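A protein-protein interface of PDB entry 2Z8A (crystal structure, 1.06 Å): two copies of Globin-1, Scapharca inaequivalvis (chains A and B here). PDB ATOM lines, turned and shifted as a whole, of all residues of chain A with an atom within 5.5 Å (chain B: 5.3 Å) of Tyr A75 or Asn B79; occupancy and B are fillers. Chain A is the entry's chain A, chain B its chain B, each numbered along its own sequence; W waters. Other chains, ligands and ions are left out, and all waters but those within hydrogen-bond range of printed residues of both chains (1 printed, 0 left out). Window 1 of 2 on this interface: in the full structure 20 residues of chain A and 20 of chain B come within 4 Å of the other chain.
ND2 of Asn B79 sits at hydrogen-bond distance from OG1 of Thr A72 (3.3 Å). OD2 of Asp B82 lies within hydrogen-bond range of OH of Tyr A75 (2.5 Å).
The side-chain amide oxygen (OE1) of Gln A78 is in hydrogen-bond range of the side-chain amino group (NZ) of Lys A29, at 3.1 Å. The side-chain hydroxyl (OG1) of Thr A72 lies within hydrogen-bond range of the backbone carbonyl oxygen (O) of Gly A68 (2.9 Å). The side-chain amide nitrogen of Gln B78 lies within hydrogen-bond range of the side-chain carboxylate of Asp B82 (3.1 Å). The side-chain amide nitrogen of Gln B83 sits at hydrogen-bond distance from the side-chain amide oxygen of Asn B79 (3.1 Å).
Among the printed residues, pairs that only touch across the chains: Gly A68 with Val B93 (3.99 Å), Ile A71 with Asn B79 (3.5 Å), Ile A71 with Gln B83 (3.8 Å), Ile A71 with Val B93 (3.9 Å), Thr A72 with Phe B97 (3.6 Å), Tyr A75 with Gln B78 (3.9 Å), Tyr A75 with Asn B79 (3.6 Å), Tyr A75 with Gln B83 (3.5 Å), Gln A78 with Tyr B75 (3.9 Å) and Asn A79 with Tyr B75 (3.5 Å).
Lys A29 touches none of the printed residues of chain B. Of the printed residues of chain B, Gly A68 touches Val B93 (3.99 Å). Ser A70 touches none of the printed residues of chain B. Of chain B, only Gln B78 (3.9 Å), Asn B79 (3.6 Å), Asp B82 (2.5 Å) and Gln B83 (3.5 Å) come within 4 Å of Tyr A75. Asn B79 touches just these residues of chain A: Ile A71, Thr A72 and Tyr A75. Of the printed residues of chain A, Gln B83 touches Ile A71 (3.8 Å) and Tyr A75 (3.5 Å). The nearest residue of chain B that does not touch Tyr A75 is Tyr B75 (4.2 Å).
Printed residues of chain B that touch a printed residue of chain A: Tyr B75, Gln B78, Asn B79, Asp B82, Gln B83, Val B93 and Phe B97. Hydrophobic or aromatic side chains of chain B within 4 Å of the printed part of chain A: Tyr B75, Val B93 and Phe B97. Of the 13 printed residues of chain A, 6 touch a printed residue of chain B. Among the printed residues, no Asp or Glu carboxylate lies within 4 Å of a Lys or Arg side-chain nitrogen of the other chain.
Tyr A75 touches Gln B78, and with the chains exchanged Gln A78 touches Tyr B75. Tyr A75 touches Asn B79, and with the chains exchanged Asn A79 touches Tyr B75. Positions printed for both chains: 74, 75, 76, 77, 78, 79 and 80. Of the 12 pairs that touch across the chains among the printed residues, 4 have their exchanged pair printed and touching as well.
Water W1 bridges OH of Tyr A75 (2.9 Å) and NE2 of Gln B83 (3.1 Å).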
ATOM      1  N   LYS A  29       6.992  -6.677  14.004  1.00  0.00           N
ATOM      2  CA  LYS A  29       7.621  -6.263  15.261  1.00  0.00           C
ATOM      3  C   LYS A  29       7.138  -4.880  15.674  1.00  0.00           C
ATOM      4  O   LYS A  29       6.918  -4.623  16.859  1.00  0.00           O
ATOM      5  CB  LYS A  29       9.145  -6.322  15.132  1.00  0.00           C
ATOM      6  CG  LYS A  29       9.672  -7.751  15.053  1.00  0.00           C
ATOM      7  CD  LYS A  29      11.188  -7.782  15.016  1.00  0.00           C
ATOM      8  CE  LYS A  29      11.753  -9.166  15.280  1.00  0.00           C
ATOM      9  NZ  LYS A  29      11.346 -10.150  14.239  1.00  0.00           N
ATOM     10  N   GLY A  68      10.291   3.381  18.629  1.00  0.00           N
ATOM     11  CA  GLY A  68      11.662   2.893  18.580  1.00  0.00           C
ATOM     12  C   GLY A  68      11.973   1.915  19.695  1.00  0.00           C
ATOM     13  O   GLY A  68      12.629   0.893  19.487  1.00  0.00           O
ATOM     14  N   SER A  70       9.746   0.032  21.207  1.00  0.00           N
ATOM     15  CA  SER A  70       8.916  -1.158  21.070  1.00  0.00           C
ATOM     16  C   SER A  70       9.464  -2.104  20.008  1.00  0.00           C
ATOM     17  O   SER A  70       9.495  -3.323  20.178  1.00  0.00           O
ATOM     18  CB  SER A  70       7.477  -0.767  20.725  1.00  0.00           C
ATOM     19  OG  SER A  70       6.879  -0.020  21.764  1.00  0.00           O
ATOM     20  N   ILE A  71       9.901  -1.538  18.882  1.00  0.00           N
ATOM     21  CA  ILE A  71      10.567  -2.355  17.869  1.00  0.00           C
ATOM     22  C   ILE A  71      11.790  -3.037  18.467  1.00  0.00           C
ATOM     23  O   ILE A  71      12.019  -4.232  18.290  1.00  0.00           O
ATOM     24  CB  ILE A  71      10.954  -1.510  16.642  1.00  0.00           C
ATOM     25  CG1 ILE A  71       9.743  -0.963  15.883  1.00  0.00           C
ATOM     26  CG2 ILE A  71      11.871  -2.288  15.714  1.00  0.00           C
ATOM     27  CD1 ILE A  71      10.058   0.158  14.923  1.00  0.00           C
ATOM     28  N   THR A  72      12.586  -2.256  19.195  1.00  0.00           N
ATOM     29  CA  THR A  72      13.825  -2.793  19.758  1.00  0.00           C
ATOM     30  C   THR A  72      13.544  -3.886  20.778  1.00  0.00           C
ATOM     31  O   THR A  72      14.276  -4.883  20.842  1.00  0.00           O
ATOM     32  CB  THR A  72      14.650  -1.639  20.359  1.00  0.00           C
ATOM     33  OG1 THR A  72      14.988  -0.735  19.292  1.00  0.00           O
ATOM     34  CG2 THR A  72      15.949  -2.143  20.952  1.00  0.00           C
ATOM     35  N   LEU A  73      12.489  -3.741  21.572  1.00  0.00           N
ATOM     36  CA  LEU A  73      12.083  -4.792  22.501  1.00  0.00           C
ATOM     37  C   LEU A  73      11.825  -6.097  21.767  1.00  0.00           C
ATOM     38  O   LEU A  73      12.197  -7.180  22.221  1.00  0.00           O
ATOM     39  CB  LEU A  73      10.842  -4.354  23.283  1.00  0.00           C
ATOM     40  CG  LEU A  73      10.313  -5.343  24.321  1.00  0.00           C
ATOM     41  CD1 LEU A  73       9.800  -4.588  25.538  1.00  0.00           C
ATOM     42  CD2 LEU A  73       9.217  -6.241  23.761  1.00  0.00           C
ATOM     43  N   MET A  74      11.163  -6.017  20.611  1.00  0.00           N
ATOM     44  CA  MET A  74      10.868  -7.241  19.871  1.00  0.00           C
ATOM     45  C   MET A  74      12.138  -7.881  19.323  1.00  0.00           C
ATOM     46  O   MET A  74      12.162  -9.100  19.123  1.00  0.00           O
ATOM     47  CB  MET A  74       9.858  -6.948  18.759  1.00  0.00           C
ATOM     48  CG  MET A  74       8.498  -6.507  19.274  1.00  0.00           C
ATOM     49  SD  MET A  74       7.594  -7.795  20.152  1.00  0.00           S
ATOM     50  CE  MET A  74       6.961  -8.748  18.769  1.00  0.00           C
ATOM     51  N   TYR A  75      13.194  -7.099  19.090  1.00  0.00           N
ATOM     52  CA  TYR A  75      14.479  -7.688  18.720  1.00  0.00           C
ATOM     53  C   TYR A  75      15.199  -8.296  19.917  1.00  0.00           C
ATOM     54  O   TYR A  75      16.029  -9.194  19.716  1.00  0.00           O
ATOM     55  CB  TYR A  75      15.387  -6.659  18.015  1.00  0.00           C
ATOM     56  CG  TYR A  75      14.957  -6.521  16.564  1.00  0.00           C
ATOM     57  CD1 TYR A  75      15.378  -7.423  15.598  1.00  0.00           C
ATOM     58  CD2 TYR A  75      14.116  -5.480  16.190  1.00  0.00           C
ATOM     59  CE1 TYR A  75      14.979  -7.291  14.279  1.00  0.00           C
ATOM     60  CE2 TYR A  75      13.716  -5.349  14.878  1.00  0.00           C
ATOM     61  CZ  TYR A  75      14.147  -6.251  13.933  1.00  0.00           C
ATOM     62  OH  TYR A  75      13.725  -6.086  12.633  1.00  0.00           O
ATOM     63  N   ALA A  76      14.914  -7.861  21.140  1.00  0.00           N
ATOM     64  CA  ALA A  76      15.389  -8.603  22.310  1.00  0.00           C
ATOM     65  C   ALA A  76      14.758  -9.991  22.348  1.00  0.00           C
ATOM     66  O   ALA A  76      15.425 -11.000  22.591  1.00  0.00           O
ATOM     67  CB  ALA A  76      15.112  -7.831  23.590  1.00  0.00           C
ATOM     68  N   LEU A  77      13.450 -10.059  22.091  1.00  0.00           N
ATOM     69  CA  LEU A  77      12.790 -11.362  22.034  1.00  0.00           C
ATOM     70  C   LEU A  77      13.320 -12.213  20.891  1.00  0.00           C
ATOM     71  O   LEU A  77      13.531 -13.416  21.061  1.00  0.00           O
ATOM     72  CB  LEU A  77      11.269 -11.177  21.932  1.00  0.00           C
ATOM     73  CG  LEU A  77      10.605 -10.461  23.112  1.00  0.00           C
ATOM     74  CD1 LEU A  77       9.094 -10.413  22.933  1.00  0.00           C
ATOM     75  CD2 LEU A  77      10.960 -11.120  24.438  1.00  0.00           C
ATOM     76  N   GLN A  78      13.552 -11.622  19.724  1.00  0.00           N
ATOM     77  CA  GLN A  78      14.149 -12.340  18.607  1.00  0.00           C
ATOM     78  C   GLN A  78      15.477 -12.979  19.004  1.00  0.00           C
ATOM     79  O   GLN A  78      15.765 -14.136  18.702  1.00  0.00           O
ATOM     80  CB  GLN A  78      14.373 -11.394  17.426  1.00  0.00           C
ATOM     81  CG  GLN A  78      14.975 -12.076  16.208  1.00  0.00           C
ATOM     82  CD  GLN A  78      13.997 -13.050  15.582  1.00  0.00           C
ATOM     83  OE1 GLN A  78      12.872 -12.672  15.251  1.00  0.00           O
ATOM     84  NE2 GLN A  78      14.425 -14.295  15.428  1.00  0.00           N
ATOM     85  N   ASN A  79      16.291 -12.182  19.683  1.00  0.00           N
ATOM     86  CA  ASN A  79      17.591 -12.608  20.195  1.00  0.00           C
ATOM     87  C   ASN A  79      17.419 -13.819  21.102  1.00  0.00           C
ATOM     88  O   ASN A  79      18.070 -14.853  20.913  1.00  0.00           O
ATOM     89  CB  ASN A  79      18.212 -11.397  20.876  1.00  0.00           C
ATOM     90  CG  ASN A  79      19.603 -11.541  21.434  1.00  0.00           C
ATOM     91  OD1 ASN A  79      20.156 -12.632  21.525  1.00  0.00           O
ATOM     92  ND2 ASN A  79      20.183 -10.404  21.822  1.00  0.00           N
ATOM     93  N   PHE A  80      16.523 -13.732  22.084  1.00  0.00           N
ATOM     94  CA  PHE A  80      16.269 -14.874  22.962  1.00  0.00           C
ATOM     95  C   PHE A  80      15.876 -16.128  22.183  1.00  0.00           C
ATOM     96  O   PHE A  80      16.403 -17.214  22.431  1.00  0.00           O
ATOM     97  CB  PHE A  80      15.169 -14.555  23.972  1.00  0.00           C
ATOM     98  CG  PHE A  80      15.479 -13.454  24.965  1.00  0.00           C
ATOM     99  CD1 PHE A  80      16.772 -13.070  25.265  1.00  0.00           C
ATOM    100  CD2 PHE A  80      14.439 -12.798  25.608  1.00  0.00           C
ATOM    101  CE1 PHE A  80      17.026 -12.065  26.180  1.00  0.00           C
ATOM    102  CE2 PHE A  80      14.680 -11.793  26.521  1.00  0.00           C
ATOM    103  CZ  PHE A  80      15.979 -11.420  26.814  1.00  0.00           C
ATOM    104  N   MET B  74      24.767  -6.935  17.389  1.00  0.00           N
ATOM    105  CA  MET B  74      24.433  -7.452  16.061  1.00  0.00           C
ATOM    106  C   MET B  74      22.925  -7.442  15.837  1.00  0.00           C
ATOM    107  O   MET B  74      22.490  -7.311  14.688  1.00  0.00           O
ATOM    108  CB  MET B  74      25.039  -8.843  15.876  1.00  0.00           C
ATOM    109  CG  MET B  74      26.557  -8.874  15.871  1.00  0.00           C
ATOM    110  SD  MET B  74      27.308  -8.083  14.432  1.00  0.00           S
ATOM    111  CE  MET B  74      27.168  -9.413  13.240  1.00  0.00           C
ATOM    112  N   TYR B  75      22.110  -7.554  16.887  1.00  0.00           N
ATOM    113  CA  TYR B  75      20.671  -7.378  16.716  1.00  0.00           C
ATOM    114  C   TYR B  75      20.275  -5.915  16.572  1.00  0.00           C
ATOM    115  O   TYR B  75      19.221  -5.650  15.982  1.00  0.00           O
ATOM    116  CB  TYR B  75      19.883  -8.027  17.876  1.00  0.00           C
ATOM    117  CG  TYR B  75      19.798  -9.523  17.641  1.00  0.00           C
ATOM    118  CD1 TYR B  75      18.867 -10.067  16.770  1.00  0.00           C
ATOM    119  CD2 TYR B  75      20.677 -10.375  18.298  1.00  0.00           C
ATOM    120  CE1 TYR B  75      18.806 -11.435  16.564  1.00  0.00           C
ATOM    121  CE2 TYR B  75      20.624 -11.735  18.096  1.00  0.00           C
ATOM    122  CZ  TYR B  75      19.685 -12.254  17.230  1.00  0.00           C
ATOM    123  OH  TYR B  75      19.656 -13.616  17.044  1.00  0.00           O
ATOM    124  N   ALA B  76      21.061  -4.965  17.063  1.00  0.00           N
ATOM    125  CA  ALA B  76      20.833  -3.562  16.705  1.00  0.00           C
ATOM    126  C   ALA B  76      21.018  -3.371  15.203  1.00  0.00           C
ATOM    127  O   ALA B  76      20.204  -2.726  14.541  1.00  0.00           O
ATOM    128  CB  ALA B  76      21.740  -2.644  17.502  1.00  0.00           C
ATOM    129  N   LEU B  77      22.085  -3.953  14.660  1.00  0.00           N
ATOM    130  CA  LEU B  77      22.293  -3.892  13.215  1.00  0.00           C
ATOM    131  C   LEU B  77      21.199  -4.626  12.450  1.00  0.00           C
ATOM    132  O   LEU B  77      20.743  -4.127  11.421  1.00  0.00           O
ATOM    133  CB  LEU B  77      23.679  -4.443  12.862  1.00  0.00           C
ATOM    134  CG  LEU B  77      24.855  -3.664  13.457  1.00  0.00           C
ATOM    135  CD1 LEU B  77      26.170  -4.276  12.993  1.00  0.00           C
ATOM    136  CD2 LEU B  77      24.800  -2.186  13.100  1.00  0.00           C
ATOM    137  N   GLN B  78      20.759  -5.786  12.921  1.00  0.00           N
ATOM    138  CA  GLN B  78      19.645  -6.487  12.293  1.00  0.00           C
ATOM    139  C   GLN B  78      18.410  -5.599  12.181  1.00  0.00           C
ATOM    140  O   GLN B  78      17.732  -5.530  11.156  1.00  0.00           O
ATOM    141  CB  GLN B  78      19.283  -7.746  13.088  1.00  0.00           C
ATOM    142  CG  GLN B  78      18.162  -8.557  12.449  1.00  0.00           C
ATOM    143  CD  GLN B  78      18.622  -9.221  11.167  1.00  0.00           C
ATOM    144  OE1 GLN B  78      19.639  -9.912  11.159  1.00  0.00           O
ATOM    145  NE2 GLN B  78      17.871  -9.009  10.094  1.00  0.00           N
ATOM    146  N   ASN B  79      18.128  -4.931  13.290  1.00  0.00           N
ATOM    147  CA  ASN B  79      17.015  -3.988  13.395  1.00  0.00           C
ATOM    148  C   ASN B  79      17.156  -2.912  12.332  1.00  0.00           C
ATOM    149  O   ASN B  79      16.238  -2.667  11.545  1.00  0.00           O
ATOM    150  CB  ASN B  79      17.013  -3.468  14.823  1.00  0.00           C
ATOM    151  CG  ASN B  79      15.891  -2.548  15.219  1.00  0.00           C
ATOM    152  OD1 ASN B  79      15.105  -2.086  14.398  1.00  0.00           O
ATOM    153  ND2 ASN B  79      15.819  -2.264  16.520  1.00  0.00           N
ATOM    154  N   PHE B  80      18.318  -2.259  12.273  1.00  0.00           N
ATOM    155  CA  PHE B  80      18.536  -1.237  11.251  1.00  0.00           C
ATOM    156  C   PHE B  80      18.305  -1.771   9.841  1.00  0.00           C
ATOM    157  O   PHE B  80      17.622  -1.144   9.023  1.00  0.00           O
ATOM    158  CB  PHE B  80      19.953  -0.680  11.339  1.00  0.00           C
ATOM    159  CG  PHE B  80      20.322   0.063  12.605  1.00  0.00           C
ATOM    160  CD1 PHE B  80      19.374   0.550  13.485  1.00  0.00           C
ATOM    161  CD2 PHE B  80      21.660   0.273  12.901  1.00  0.00           C
ATOM    162  CE1 PHE B  80      19.743   1.230  14.632  1.00  0.00           C
ATOM    163  CE2 PHE B  80      22.041   0.946  14.044  1.00  0.00           C
ATOM    164  CZ  PHE B  80      21.080   1.427  14.910  1.00  0.00           C
ATOM    165  N   ILE B  81      18.884  -2.927   9.533  1.00  0.00           N
ATOM    166  CA  ILE B  81      18.740  -3.493   8.191  1.00  0.00           C
ATOM    167  C   ILE B  81      17.273  -3.742   7.874  1.00  0.00           C
ATOM    168  O   ILE B  81      16.796  -3.480   6.769  1.00  0.00           O
ATOM    169  CB  ILE B  81      19.580  -4.777   8.066  1.00  0.00           C
ATOM    170  CG1 ILE B  81      21.085  -4.514   8.146  1.00  0.00           C
ATOM    171  CG2 ILE B  81      19.212  -5.532   6.802  1.00  0.00           C
ATOM    172  CD1 ILE B  81      21.622  -3.718   6.971  1.00  0.00           C
ATOM    173  N   ASP B  82      16.530  -4.242   8.860  1.00  0.00           N
ATOM    174  CA  ASP B  82      15.121  -4.536   8.628  1.00  0.00           C
ATOM    175  C   ASP B  82      14.288  -3.268   8.454  1.00  0.00           C
ATOM    176  O   ASP B  82      13.197  -3.368   7.880  1.00  0.00           O
ATOM    177  CB  ASP B  82      14.576  -5.380   9.780  1.00  0.00           C
ATOM    178  CG  ASP B  82      15.099  -6.797   9.808  1.00  0.00           C
ATOM    179  OD1 ASP B  82      15.651  -7.290   8.803  1.00  0.00           O
ATOM    180  OD2 ASP B  82      14.948  -7.452  10.865  1.00  0.00           O
ATOM    181  N   GLN B  83      14.758  -2.115   8.919  1.00  0.00           N
ATOM    182  CA  GLN B  83      13.998  -0.876   8.796  1.00  0.00           C
ATOM    183  C   GLN B  83      14.381  -0.051   7.569  1.00  0.00           C
ATOM    184  O   GLN B  83      13.833   1.041   7.389  1.00  0.00           O
ATOM    185  CB  GLN B  83      14.172   0.026  10.023  1.00  0.00           C
ATOM    186  CG  GLN B  83      13.930  -0.578  11.380  1.00  0.00           C
ATOM    187  CD  GLN B  83      12.806  -1.587  11.426  1.00  0.00           C
ATOM    188  OE1 GLN B  83      11.749  -1.392  10.829  1.00  0.00           O
ATOM    189  NE2 GLN B  83      13.043  -2.673  12.154  1.00  0.00           N
ATOM    190  N   VAL B  93      14.465   3.944  15.543  1.00  0.00           N
ATOM    191  CA  VAL B  93      15.353   2.993  16.226  1.00  0.00           C
ATOM    192  C   VAL B  93      16.779   3.534  16.282  1.00  0.00           C
ATOM    193  O   VAL B  93      17.483   3.316  17.280  1.00  0.00           O
ATOM    194  CB  VAL B  93      15.321   1.588  15.598  1.00  0.00           C
ATOM    195  CG1 VAL B  93      13.914   1.005  15.716  1.00  0.00           C
ATOM    196  CG2 VAL B  93      15.772   1.575  14.150  1.00  0.00           C
ATOM    197  N   PHE B  97      19.076   3.974  19.832  1.00  0.00           N
ATOM    198  CA  PHE B  97      20.449   3.543  20.107  1.00  0.00           C
ATOM    199  C   PHE B  97      21.393   4.727  20.242  1.00  0.00           C
ATOM    200  O   PHE B  97      22.399   4.639  20.956  1.00  0.00           O
ATOM    201  CB  PHE B  97      20.944   2.577  19.024  1.00  0.00           C
ATOM    202  CG  PHE B  97      20.267   1.216  19.138  1.00  0.00           C
ATOM    203  CD1 PHE B  97      20.557   0.375  20.196  1.00  0.00           C
ATOM    204  CD2 PHE B  97      19.354   0.806  18.187  1.00  0.00           C
ATOM    205  CE1 PHE B  97      19.944  -0.863  20.307  1.00  0.00           C
ATOM    206  CE2 PHE B  97      18.737  -0.426  18.290  1.00  0.00           C
ATOM    207  CZ  PHE B  97      19.031  -1.260  19.351  1.00  0.00           C
HETATM  208  O   HOH W   1      11.067  -5.039  11.955  1.00  0.00           O
